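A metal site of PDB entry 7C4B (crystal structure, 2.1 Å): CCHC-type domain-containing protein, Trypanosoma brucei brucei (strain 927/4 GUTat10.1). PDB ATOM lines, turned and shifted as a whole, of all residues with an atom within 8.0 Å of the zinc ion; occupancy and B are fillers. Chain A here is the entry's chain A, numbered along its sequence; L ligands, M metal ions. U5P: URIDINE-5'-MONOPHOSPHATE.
The backbone carbonyl oxygen (O) of Ala 263 is in hydrogen-bond range of the backbone NH (N) of Cys 258, 2.8 Å away. The backbone NH of Phe 260 sits close to the side-chain sulfur of Cys 258 (3.4 Å). The side-chain sulfur of Cys 271 sits close to the backbone NH of Lys 274. The side-chain sulfur (SG) of Cys 261 sits close to the backbone NH (N) of Ala 263 (3.6 Å). The side-chain sulfur (SG) of Cys 271 lies close to the backbone NH (N) of Lys 273, 3.5 Å away.
The zinc ion is bound by NE2 of His 266 (2.2 Å), SG of Cys 261 (2.2 Å), SG of Cys 271 (2.3 Å) and SG of Cys 258 (2.3 Å). The zinc ion has four donor atoms within binding distance.
Of the 19 residues printed, 4 come within 4 Å of the zinc ion. The nearest printed residue that does not touch the zinc ion is Phe 260 (4.6 Å).
A ring nitrogen (NE2) of His 266 sits close to an oxygen (O4) of the ligand, at 3.4 Å. The backbone NH (N) of Phe 272 lies within hydrogen-bond range of an oxygen (O4) of the ligand, at 2.8 Å. An oxygen (O2') of the ligand lies within hydrogen-bond range of the side-chain carboxylate (OE1) of Glu 270 (3.4 Å). The backbone carbonyl oxygen (O) of Glu 270 sits at hydrogen-bond distance from a nitrogen (N3) of the ligand (2.7 Å). O of Gly 265 is in hydrogen-bond range of O2' of the ligand (3.4 Å).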
ATOM      1  N   GLY A 257      24.940 -14.554 -22.709  1.00  0.00           N
ATOM      2  CA  GLY A 257      24.595 -15.268 -21.503  1.00  0.00           C
ATOM      3  C   GLY A 257      25.806 -15.374 -20.601  1.00  0.00           C
ATOM      4  O   GLY A 257      26.863 -14.806 -20.874  1.00  0.00           O
ATOM      5  N   CYS A 258      25.631 -16.122 -19.515  1.00  0.00           N
ATOM      6  CA  CYS A 258      26.683 -16.296 -18.520  1.00  0.00           C
ATOM      7  C   CYS A 258      27.727 -17.294 -19.027  1.00  0.00           C
ATOM      8  O   CYS A 258      27.388 -18.443 -19.333  1.00  0.00           O
ATOM      9  CB  CYS A 258      26.105 -16.768 -17.194  1.00  0.00           C
ATOM     10  SG  CYS A 258      27.342 -17.019 -15.912  1.00  0.00           S
ATOM     11  N   HIS A 259      28.975 -16.852 -19.113  1.00  0.00           N
ATOM     12  CA  HIS A 259      30.045 -17.740 -19.573  1.00  0.00           C
ATOM     13  C   HIS A 259      30.358 -18.835 -18.563  1.00  0.00           C
ATOM     14  O   HIS A 259      31.011 -19.816 -18.929  1.00  0.00           O
ATOM     15  CB  HIS A 259      31.310 -16.941 -19.869  1.00  0.00           C
ATOM     16  CG  HIS A 259      31.154 -15.935 -20.970  1.00  0.00           C
ATOM     17  ND1 HIS A 259      32.170 -15.070 -21.339  1.00  0.00           N
ATOM     18  CD2 HIS A 259      30.107 -15.651 -21.770  1.00  0.00           C
ATOM     19  CE1 HIS A 259      31.746 -14.301 -22.323  1.00  0.00           C
ATOM     20  NE2 HIS A 259      30.503 -14.626 -22.607  1.00  0.00           N
ATOM     21  N   PHE A 260      29.930 -18.696 -17.320  1.00  0.00           N
ATOM     22  CA  PHE A 260      30.274 -19.679 -16.285  1.00  0.00           C
ATOM     23  C   PHE A 260      29.278 -20.837 -16.247  1.00  0.00           C
ATOM     24  O   PHE A 260      29.681 -22.003 -16.344  1.00  0.00           O
ATOM     25  CB  PHE A 260      30.366 -19.011 -14.916  1.00  0.00           C
ATOM     26  CG  PHE A 260      30.951 -19.900 -13.852  1.00  0.00           C
ATOM     27  CD1 PHE A 260      32.320 -20.034 -13.731  1.00  0.00           C
ATOM     28  CD2 PHE A 260      30.129 -20.610 -12.991  1.00  0.00           C
ATOM     29  CE1 PHE A 260      32.868 -20.860 -12.766  1.00  0.00           C
ATOM     30  CE2 PHE A 260      30.669 -21.431 -12.028  1.00  0.00           C
ATOM     31  CZ  PHE A 260      32.042 -21.557 -11.909  1.00  0.00           C
ATOM     32  N   CYS A 261      27.994 -20.545 -16.103  1.00  0.00           N
ATOM     33  CA  CYS A 261      26.986 -21.592 -16.009  1.00  0.00           C
ATOM     34  C   CYS A 261      26.213 -21.796 -17.298  1.00  0.00           C
ATOM     35  O   CYS A 261      25.539 -22.833 -17.441  1.00  0.00           O
ATOM     36  CB  CYS A 261      26.004 -21.294 -14.861  1.00  0.00           C
ATOM     37  SG  CYS A 261      24.932 -19.872 -15.141  1.00  0.00           S
ATOM     38  N   GLY A 262      26.274 -20.858 -18.242  1.00  0.00           N
ATOM     39  CA  GLY A 262      25.602 -20.997 -19.518  1.00  0.00           C
ATOM     40  C   GLY A 262      24.210 -20.428 -19.581  1.00  0.00           C
ATOM     41  O   GLY A 262      23.609 -20.401 -20.670  1.00  0.00           O
ATOM     42  N   ALA A 263      23.654 -19.970 -18.455  1.00  0.00           N
ATOM     43  CA  ALA A 263      22.292 -19.466 -18.441  1.00  0.00           C
ATOM     44  C   ALA A 263      22.226 -18.033 -18.969  1.00  0.00           C
ATOM     45  O   ALA A 263      23.166 -17.256 -18.832  1.00  0.00           O
ATOM     46  CB  ALA A 263      21.720 -19.521 -17.018  1.00  0.00           C
ATOM     47  N   LYS A 264      21.092 -17.704 -19.576  1.00  0.00           N
ATOM     48  CA  LYS A 264      20.831 -16.347 -20.030  1.00  0.00           C
ATOM     49  C   LYS A 264      20.233 -15.531 -18.893  1.00  0.00           C
ATOM     50  O   LYS A 264      19.709 -16.067 -17.915  1.00  0.00           O
ATOM     51  CB  LYS A 264      19.901 -16.354 -21.234  1.00  0.00           C
ATOM     52  CG  LYS A 264      20.375 -17.251 -22.367  1.00  0.00           C
ATOM     53  CD  LYS A 264      19.491 -17.159 -23.593  1.00  0.00           C
ATOM     54  CE  LYS A 264      20.057 -18.015 -24.728  1.00  0.00           C
ATOM     55  NZ  LYS A 264      19.256 -17.908 -25.978  1.00  0.00           N
ATOM     56  N   GLY A 265      20.336 -14.201 -19.019  1.00  0.00           N
ATOM     57  CA  GLY A 265      19.782 -13.286 -18.054  1.00  0.00           C
ATOM     58  C   GLY A 265      20.804 -12.640 -17.136  1.00  0.00           C
ATOM     59  O   GLY A 265      20.479 -11.643 -16.490  1.00  0.00           O
ATOM     60  N   HIS A 266      22.017 -13.170 -17.061  1.00  0.00           N
ATOM     61  CA  HIS A 266      23.044 -12.587 -16.216  1.00  0.00           C
ATOM     62  C   HIS A 266      24.419 -12.909 -16.792  1.00  0.00           C
ATOM     63  O   HIS A 266      24.567 -13.831 -17.608  1.00  0.00           O
ATOM     64  CB  HIS A 266      22.952 -13.095 -14.767  1.00  0.00           C
ATOM     65  CG  HIS A 266      23.276 -14.540 -14.609  1.00  0.00           C
ATOM     66  ND1 HIS A 266      22.324 -15.531 -14.682  1.00  0.00           N
ATOM     67  CD2 HIS A 266      24.446 -15.178 -14.390  1.00  0.00           C
ATOM     68  CE1 HIS A 266      22.888 -16.718 -14.511  1.00  0.00           C
ATOM     69  NE2 HIS A 266      24.188 -16.522 -14.328  1.00  0.00           N
ATOM     70  N   THR A 267      25.407 -12.141 -16.374  1.00  0.00           N
ATOM     71  CA  THR A 267      26.782 -12.319 -16.810  1.00  0.00           C
ATOM     72  C   THR A 267      27.585 -13.061 -15.750  1.00  0.00           C
ATOM     73  O   THR A 267      27.093 -13.386 -14.664  1.00  0.00           O
ATOM     74  CB  THR A 267      27.425 -10.969 -17.138  1.00  0.00           C
ATOM     75  OG1 THR A 267      27.543 -10.190 -15.935  1.00  0.00           O
ATOM     76  CG2 THR A 267      26.581 -10.197 -18.147  1.00  0.00           C
ATOM     77  N   GLU A 268      28.852 -13.333 -16.081  1.00  0.00           N
ATOM     78  CA  GLU A 268      29.711 -14.105 -15.189  1.00  0.00           C
ATOM     79  C   GLU A 268      29.914 -13.393 -13.853  1.00  0.00           C
ATOM     80  O   GLU A 268      29.906 -14.032 -12.791  1.00  0.00           O
ATOM     81  CB  GLU A 268      31.048 -14.367 -15.872  1.00  0.00           C
ATOM     82  CG  GLU A 268      31.960 -15.354 -15.168  1.00  0.00           C
ATOM     83  CD  GLU A 268      33.134 -15.758 -16.029  1.00  0.00           C
ATOM     84  OE1 GLU A 268      33.284 -15.196 -17.134  1.00  0.00           O
ATOM     85  OE2 GLU A 268      33.919 -16.640 -15.598  1.00  0.00           O
ATOM     86  N   ALA A 269      30.076 -12.068 -13.890  1.00  0.00           N
ATOM     87  CA  ALA A 269      30.295 -11.304 -12.657  1.00  0.00           C
ATOM     88  C   ALA A 269      29.080 -11.342 -11.738  1.00  0.00           C
ATOM     89  O   ALA A 269      29.235 -11.118 -10.528  1.00  0.00           O
ATOM     90  CB  ALA A 269      30.656  -9.860 -12.996  1.00  0.00           C
ATOM     91  N   GLU A 270      27.892 -11.600 -12.267  1.00  0.00           N
ATOM     92  CA  GLU A 270      26.672 -11.676 -11.472  1.00  0.00           C
ATOM     93  C   GLU A 270      26.267 -13.094 -11.133  1.00  0.00           C
ATOM     94  O   GLU A 270      25.241 -13.298 -10.478  1.00  0.00           O
ATOM     95  CB  GLU A 270      25.520 -10.982 -12.218  1.00  0.00           C
ATOM     96  CG  GLU A 270      25.899  -9.687 -12.896  1.00  0.00           C
ATOM     97  CD  GLU A 270      24.874  -9.261 -13.926  1.00  0.00           C
ATOM     98  OE1 GLU A 270      23.900 -10.009 -14.149  1.00  0.00           O
ATOM     99  OE2 GLU A 270      25.042  -8.176 -14.526  1.00  0.00           O
ATOM    100  N   CYS A 271      27.044 -14.090 -11.575  1.00  0.00           N
ATOM    101  CA  CYS A 271      26.620 -15.485 -11.458  1.00  0.00           C
ATOM    102  C   CYS A 271      26.673 -15.930  -9.995  1.00  0.00           C
ATOM    103  O   CYS A 271      27.738 -15.901  -9.357  1.00  0.00           O
ATOM    104  CB  CYS A 271      27.511 -16.373 -12.316  1.00  0.00           C
ATOM    105  SG  CYS A 271      27.006 -18.105 -12.337  1.00  0.00           S
ATOM    106  N   PHE A 272      25.513 -16.354  -9.478  1.00  0.00           N
ATOM    107  CA  PHE A 272      25.474 -16.885  -8.115  1.00  0.00           C
ATOM    108  C   PHE A 272      26.287 -18.168  -7.998  1.00  0.00           C
ATOM    109  O   PHE A 272      26.983 -18.380  -7.001  1.00  0.00           O
ATOM    110  CB  PHE A 272      24.021 -17.142  -7.698  1.00  0.00           C
ATOM    111  CG  PHE A 272      23.158 -15.918  -7.679  1.00  0.00           C
ATOM    112  CD1 PHE A 272      23.699 -14.674  -7.379  1.00  0.00           C
ATOM    113  CD2 PHE A 272      21.806 -15.996  -7.969  1.00  0.00           C
ATOM    114  CE1 PHE A 272      22.899 -13.547  -7.355  1.00  0.00           C
ATOM    115  CE2 PHE A 272      21.006 -14.872  -7.954  1.00  0.00           C
ATOM    116  CZ  PHE A 272      21.551 -13.642  -7.649  1.00  0.00           C
ATOM    117  N   LYS A 273      26.223 -19.027  -9.013  1.00  0.00           N
ATOM    118  CA  LYS A 273      26.904 -20.317  -8.941  1.00  0.00           C
ATOM    119  C   LYS A 273      28.416 -20.154  -8.909  1.00  0.00           C
ATOM    120  O   LYS A 273      29.105 -20.914  -8.217  1.00  0.00           O
ATOM    121  CB  LYS A 273      26.479 -21.205 -10.116  1.00  0.00           C
ATOM    122  CG  LYS A 273      24.980 -21.433 -10.209  1.00  0.00           C
ATOM    123  CD  LYS A 273      24.646 -22.425 -11.312  1.00  0.00           C
ATOM    124  CE  LYS A 273      23.146 -22.463 -11.568  1.00  0.00           C
ATOM    125  NZ  LYS A 273      22.639 -21.159 -12.085  1.00  0.00           N
ATOM    126  N   LYS A 274      28.949 -19.180  -9.649  1.00  0.00           N
ATOM    127  CA  LYS A 274      30.387 -18.954  -9.600  1.00  0.00           C
ATOM    128  C   LYS A 274      30.801 -18.401  -8.244  1.00  0.00           C
ATOM    129  O   LYS A 274      31.861 -18.773  -7.719  1.00  0.00           O
ATOM    130  CB  LYS A 274      30.811 -17.989 -10.711  1.00  0.00           C
ATOM    131  CG  LYS A 274      32.317 -17.837 -10.835  1.00  0.00           C
ATOM    132  CD  LYS A 274      32.701 -16.817 -11.893  1.00  0.00           C
ATOM    133  CE  LYS A 274      34.217 -16.667 -11.963  1.00  0.00           C
ATOM    134  NZ  LYS A 274      34.638 -15.590 -12.891  1.00  0.00           N
ATOM    135  N   GLN A 275      29.985 -17.526  -7.654  1.00  0.00           N
ATOM    136  CA  GLN A 275      30.311 -16.982  -6.340  1.00  0.00           C
ATOM    137  C   GLN A 275      30.170 -18.027  -5.245  1.00  0.00           C
ATOM    138  O   GLN A 275      31.024 -18.145  -4.371  1.00  0.00           O
ATOM    139  CB  GLN A 275      29.430 -15.764  -6.044  1.00  0.00           C
HETATM  140  N1  U5P L   1      20.692 -13.272 -11.317  1.00  0.00           N
HETATM  141  C2  U5P L   1      22.016 -13.074 -10.974  1.00  0.00           C
HETATM  142  N3  U5P L   1      22.781 -14.214 -10.920  1.00  0.00           N
HETATM  143  C4  U5P L   1      22.365 -15.504 -11.168  1.00  0.00           C
HETATM  144  C5  U5P L   1      20.986 -15.634 -11.515  1.00  0.00           C
HETATM  145  C6  U5P L   1      20.211 -14.538 -11.575  1.00  0.00           C
HETATM  146  O2  U5P L   1      22.473 -11.970 -10.734  1.00  0.00           O
HETATM  147  O4  U5P L   1      23.178 -16.429 -11.072  1.00  0.00           O
HETATM  148  C1' U5P L   1      19.827 -12.089 -11.389  1.00  0.00           C
HETATM  149  C2' U5P L   1      19.614 -11.556 -12.803  1.00  0.00           C
HETATM  150  O2' U5P L   1      20.676 -10.733 -13.219  1.00  0.00           O
HETATM  151  C3' U5P L   1      18.278 -10.839 -12.651  1.00  0.00           C
HETATM  152  C4' U5P L   1      17.530 -11.716 -11.644  1.00  0.00           C
HETATM  153  O3' U5P L   1      18.486  -9.547 -12.082  1.00  0.00           O
HETATM  154  O4' U5P L   1      18.542 -12.437 -10.903  1.00  0.00           O
HETATM  155  C5' U5P L   1      16.554 -12.711 -12.247  1.00  0.00           C
HETATM  156  O5' U5P L   1      17.212 -13.698 -13.024  1.00  0.00           O
HETATM  157  P   U5P L   1      16.499 -15.097 -13.338  1.00  0.00           P
HETATM  158  O1P U5P L   1      17.582 -16.080 -13.617  1.00  0.00           O
HETATM  159  O2P U5P L   1      15.480 -14.836 -14.374  1.00  0.00           O
HETATM  160  O3P U5P L   1      15.802 -15.532 -12.115  1.00  0.00           O
HETATM  161 ZN    ZN M   1      25.870 -17.993 -14.363  1.00  0.00          ZN
